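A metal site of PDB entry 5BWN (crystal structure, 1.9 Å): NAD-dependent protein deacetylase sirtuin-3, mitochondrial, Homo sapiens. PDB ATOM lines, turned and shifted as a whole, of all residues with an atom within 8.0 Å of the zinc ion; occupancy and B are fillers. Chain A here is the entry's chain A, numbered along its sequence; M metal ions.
The zinc ion is bound by the side-chain sulfur of Cys 190 (2.4 Å), the side-chain sulfur of Cys 193 (2.4 Å), the side-chain sulfur of Cys 166 (2.4 Å) and the side-chain sulfur of Cys 169 (2.5 Å).
N of Cys 190 sits at hydrogen-bond distance from O of Gly 195, 2.8 Å away. The backbone NH (N) of Val 192 sits close to the side-chain sulfur (SG) of Cys 190, at 3.3 Å. The backbone NH of Gly 195 lies close to the side-chain sulfur of Cys 193 (3.4 Å). The backbone NH (N) of Val 168 lies close to the side-chain sulfur (SG) of Cys 166, 3.2 Å away. N of Cys 166 is in hydrogen-bond range of O of Arg 171, 2.9 Å away. The side-chain sulfur of Cys 169 sits close to the guanidinium group of Arg 171 (3.6 Å).
Of the 18 residues printed, 4 come within 4 Å of the zinc ion. The nearest printed residue that does not touch the zinc ion is Gly 195 (4.5 Å).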
ATOM      1  N   THR A 165     -14.489  -8.466   6.895  1.00  0.00           N
ATOM      2  CA  THR A 165     -15.517  -8.611   5.876  1.00  0.00           C
ATOM      3  C   THR A 165     -16.784  -7.909   6.341  1.00  0.00           C
ATOM      4  O   THR A 165     -17.234  -8.129   7.467  1.00  0.00           O
ATOM      5  CB  THR A 165     -15.794 -10.096   5.603  1.00  0.00           C
ATOM      6  OG1 THR A 165     -14.580 -10.762   5.241  1.00  0.00           O
ATOM      7  CG2 THR A 165     -16.774 -10.282   4.458  1.00  0.00           C
ATOM      8  N   CYS A 166     -17.359  -7.048   5.480  1.00  0.00           N
ATOM      9  CA  CYS A 166     -18.644  -6.448   5.819  1.00  0.00           C
ATOM     10  C   CYS A 166     -19.693  -7.531   5.926  1.00  0.00           C
ATOM     11  O   CYS A 166     -19.891  -8.314   4.986  1.00  0.00           O
ATOM     12  CB  CYS A 166     -19.124  -5.399   4.778  1.00  0.00           C
ATOM     13  SG  CYS A 166     -20.683  -4.704   5.383  1.00  0.00           S
ATOM     14  N   THR A 167     -20.381  -7.579   7.075  1.00  0.00           N
ATOM     15  CA  THR A 167     -21.436  -8.552   7.291  1.00  0.00           C
ATOM     16  C   THR A 167     -22.688  -8.294   6.462  1.00  0.00           C
ATOM     17  O   THR A 167     -23.591  -9.132   6.485  1.00  0.00           O
ATOM     18  CB  THR A 167     -21.835  -8.581   8.759  1.00  0.00           C
ATOM     19  OG1 THR A 167     -22.316  -7.275   9.150  1.00  0.00           O
ATOM     20  CG2 THR A 167     -20.646  -9.001   9.620  1.00  0.00           C
ATOM     21  N   VAL A 168     -22.764  -7.158   5.767  1.00  0.00           N
ATOM     22  CA  VAL A 168     -23.937  -6.807   4.963  1.00  0.00           C
ATOM     23  C   VAL A 168     -23.671  -6.952   3.474  1.00  0.00           C
ATOM     24  O   VAL A 168     -24.373  -7.682   2.781  1.00  0.00           O
ATOM     25  CB  VAL A 168     -24.464  -5.403   5.317  1.00  0.00           C
ATOM     26  CG1 VAL A 168     -25.581  -5.002   4.355  1.00  0.00           C
ATOM     27  CG2 VAL A 168     -25.005  -5.350   6.759  1.00  0.00           C
ATOM     28  N   CYS A 169     -22.679  -6.214   2.948  1.00  0.00           N
ATOM     29  CA  CYS A 169     -22.394  -6.288   1.512  1.00  0.00           C
ATOM     30  C   CYS A 169     -21.283  -7.280   1.162  1.00  0.00           C
ATOM     31  O   CYS A 169     -21.028  -7.516  -0.016  1.00  0.00           O
ATOM     32  CB  CYS A 169     -22.029  -4.908   0.935  1.00  0.00           C
ATOM     33  SG  CYS A 169     -20.408  -4.268   1.414  1.00  0.00           S
ATOM     34  N   GLN A 170     -20.611  -7.856   2.164  1.00  0.00           N
ATOM     35  CA  GLN A 170     -19.584  -8.876   1.980  1.00  0.00           C
ATOM     36  C   GLN A 170     -18.267  -8.335   1.433  1.00  0.00           C
ATOM     37  O   GLN A 170     -17.412  -9.108   1.052  1.00  0.00           O
ATOM     38  CB  GLN A 170     -20.046 -10.010   1.050  1.00  0.00           C
ATOM     39  CG  GLN A 170     -21.316 -10.709   1.473  1.00  0.00           C
ATOM     40  CD  GLN A 170     -21.240 -11.279   2.881  1.00  0.00           C
ATOM     41  OE1 GLN A 170     -20.199 -11.788   3.312  1.00  0.00           O
ATOM     42  NE2 GLN A 170     -22.337 -11.176   3.607  1.00  0.00           N
ATOM     43  N   ARG A 171     -18.067  -7.022   1.407  1.00  0.00           N
ATOM     44  CA  ARG A 171     -16.801  -6.486   0.911  1.00  0.00           C
ATOM     45  C   ARG A 171     -15.633  -6.855   1.847  1.00  0.00           C
ATOM     46  O   ARG A 171     -15.741  -6.717   3.061  1.00  0.00           O
ATOM     47  CB  ARG A 171     -16.904  -4.970   0.768  1.00  0.00           C
ATOM     48  CG  ARG A 171     -15.585  -4.273   0.542  1.00  0.00           C
ATOM     49  CD  ARG A 171     -15.831  -2.840   0.056  1.00  0.00           C
ATOM     50  NE  ARG A 171     -16.123  -2.789  -1.381  1.00  0.00           N
ATOM     51  CZ  ARG A 171     -17.335  -2.738  -1.916  1.00  0.00           C
ATOM     52  NH1 ARG A 171     -17.457  -2.673  -3.237  1.00  0.00           N
ATOM     53  NH2 ARG A 171     -18.437  -2.798  -1.164  1.00  0.00           N
ATOM     54  N   PRO A 172     -14.474  -7.252   1.302  1.00  0.00           N
ATOM     55  CA  PRO A 172     -13.330  -7.549   2.169  1.00  0.00           C
ATOM     56  C   PRO A 172     -12.462  -6.340   2.423  1.00  0.00           C
ATOM     57  O   PRO A 172     -12.344  -5.428   1.596  1.00  0.00           O
ATOM     58  CB  PRO A 172     -12.573  -8.618   1.368  1.00  0.00           C
ATOM     59  CG  PRO A 172     -12.841  -8.274  -0.024  1.00  0.00           C
ATOM     60  CD  PRO A 172     -14.228  -7.682  -0.079  1.00  0.00           C
ATOM     61  N   PHE A 173     -11.825  -6.329   3.590  1.00  0.00           N
ATOM     62  CA  PHE A 173     -10.937  -5.242   3.972  1.00  0.00           C
ATOM     63  C   PHE A 173      -9.668  -5.797   4.594  1.00  0.00           C
ATOM     64  O   PHE A 173      -9.685  -6.901   5.159  1.00  0.00           O
ATOM     65  CB  PHE A 173     -11.603  -4.291   4.976  1.00  0.00           C
ATOM     66  CG  PHE A 173     -12.852  -3.639   4.450  1.00  0.00           C
ATOM     67  CD1 PHE A 173     -12.776  -2.471   3.710  1.00  0.00           C
ATOM     68  CD2 PHE A 173     -14.092  -4.211   4.675  1.00  0.00           C
ATOM     69  CE1 PHE A 173     -13.925  -1.872   3.213  1.00  0.00           C
ATOM     70  CE2 PHE A 173     -15.249  -3.611   4.183  1.00  0.00           C
ATOM     71  CZ  PHE A 173     -15.157  -2.447   3.449  1.00  0.00           C
ATOM     72  N   ARG A 189     -17.689   0.074  11.073  1.00  0.00           N
ATOM     73  CA  ARG A 189     -18.736   0.007  10.073  1.00  0.00           C
ATOM     74  C   ARG A 189     -18.164   0.243   8.686  1.00  0.00           C
ATOM     75  O   ARG A 189     -17.123   0.883   8.516  1.00  0.00           O
ATOM     76  CB  ARG A 189     -19.873   0.987  10.393  1.00  0.00           C
ATOM     77  CG  ARG A 189     -20.648   0.515  11.603  1.00  0.00           C
ATOM     78  CD  ARG A 189     -21.802   1.355  11.975  1.00  0.00           C
ATOM     79  NE  ARG A 189     -22.493   0.719  13.094  1.00  0.00           N
ATOM     80  CZ  ARG A 189     -23.412  -0.226  12.962  1.00  0.00           C
ATOM     81  NH1 ARG A 189     -23.790  -0.643  11.750  1.00  0.00           N
ATOM     82  NH2 ARG A 189     -23.967  -0.759  14.043  1.00  0.00           N
ATOM     83  N   CYS A 190     -18.885  -0.271   7.706  1.00  0.00           N
ATOM     84  CA  CYS A 190     -18.425  -0.380   6.341  1.00  0.00           C
ATOM     85  C   CYS A 190     -18.524   0.970   5.637  1.00  0.00           C
ATOM     86  O   CYS A 190     -19.568   1.613   5.694  1.00  0.00           O
ATOM     87  CB  CYS A 190     -19.283  -1.394   5.612  1.00  0.00           C
ATOM     88  SG  CYS A 190     -18.906  -1.593   3.868  1.00  0.00           S
ATOM     89  N   PRO A 191     -17.476   1.426   4.933  1.00  0.00           N
ATOM     90  CA  PRO A 191     -17.573   2.710   4.218  1.00  0.00           C
ATOM     91  C   PRO A 191     -18.516   2.673   3.028  1.00  0.00           C
ATOM     92  O   PRO A 191     -18.889   3.732   2.520  1.00  0.00           O
ATOM     93  CB  PRO A 191     -16.130   2.996   3.790  1.00  0.00           C
ATOM     94  CG  PRO A 191     -15.513   1.654   3.685  1.00  0.00           C
ATOM     95  CD  PRO A 191     -16.156   0.796   4.730  1.00  0.00           C
ATOM     96  N   VAL A 192     -18.929   1.489   2.575  1.00  0.00           N
ATOM     97  CA  VAL A 192     -19.851   1.366   1.452  1.00  0.00           C
ATOM     98  C   VAL A 192     -21.314   1.312   1.918  1.00  0.00           C
ATOM     99  O   VAL A 192     -22.139   2.102   1.436  1.00  0.00           O
ATOM    100  CB  VAL A 192     -19.501   0.117   0.610  1.00  0.00           C
ATOM    101  CG1 VAL A 192     -20.534  -0.093  -0.497  1.00  0.00           C
ATOM    102  CG2 VAL A 192     -18.096   0.265   0.025  1.00  0.00           C
ATOM    103  N   CYS A 193     -21.676   0.382   2.833  1.00  0.00           N
ATOM    104  CA  CYS A 193     -23.086   0.262   3.206  1.00  0.00           C
ATOM    105  C   CYS A 193     -23.377   0.572   4.663  1.00  0.00           C
ATOM    106  O   CYS A 193     -24.552   0.598   5.030  1.00  0.00           O
ATOM    107  CB  CYS A 193     -23.606  -1.148   2.895  1.00  0.00           C
ATOM    108  SG  CYS A 193     -22.993  -2.445   3.965  1.00  0.00           S
ATOM    109  N   THR A 194     -22.356   0.849   5.486  1.00  0.00           N
ATOM    110  CA  THR A 194     -22.424   1.110   6.931  1.00  0.00           C
ATOM    111  C   THR A 194     -22.771  -0.120   7.754  1.00  0.00           C
ATOM    112  O   THR A 194     -23.001   0.010   8.963  1.00  0.00           O
ATOM    113  CB  THR A 194     -23.419   2.221   7.297  1.00  0.00           C
ATOM    114  OG1 THR A 194     -24.760   1.762   7.093  1.00  0.00           O
ATOM    115  CG2 THR A 194     -23.184   3.464   6.441  1.00  0.00           C
ATOM    116  N   GLY A 195     -22.795  -1.310   7.158  1.00  0.00           N
ATOM    117  CA  GLY A 195     -22.963  -2.522   7.941  1.00  0.00           C
ATOM    118  C   GLY A 195     -21.743  -2.832   8.794  1.00  0.00           C
ATOM    119  O   GLY A 195     -20.634  -2.319   8.582  1.00  0.00           O
ATOM    120  N   VAL A 196     -21.947  -3.696   9.777  1.00  0.00           N
ATOM    121  CA  VAL A 196     -20.894  -4.039  10.722  1.00  0.00           C
ATOM    122  C   VAL A 196     -19.819  -4.864  10.028  1.00  0.00           C
ATOM    123  O   VAL A 196     -20.110  -5.883   9.386  1.00  0.00           O
ATOM    124  CB  VAL A 196     -21.478  -4.789  11.928  1.00  0.00           C
ATOM    125  CG1 VAL A 196     -20.355  -5.364  12.834  1.00  0.00           C
ATOM    126  CG2 VAL A 196     -22.368  -3.866  12.734  1.00  0.00           C
ATOM    127  N   VAL A 197     -18.565  -4.434  10.178  1.00  0.00           N
ATOM    128  CA  VAL A 197     -17.429  -5.157   9.632  1.00  0.00           C
ATOM    129  C   VAL A 197     -16.927  -6.119  10.710  1.00  0.00           C
ATOM    130  O   VAL A 197     -16.729  -5.741  11.868  1.00  0.00           O
ATOM    131  CB  VAL A 197     -16.323  -4.170   9.180  1.00  0.00           C
ATOM    132  CG1 VAL A 197     -15.128  -4.900   8.598  1.00  0.00           C
ATOM    133  CG2 VAL A 197     -16.873  -3.255   8.121  1.00  0.00           C
HETATM  134 ZN    ZN M   1     -20.715  -3.092   3.595  1.00  0.00          ZN
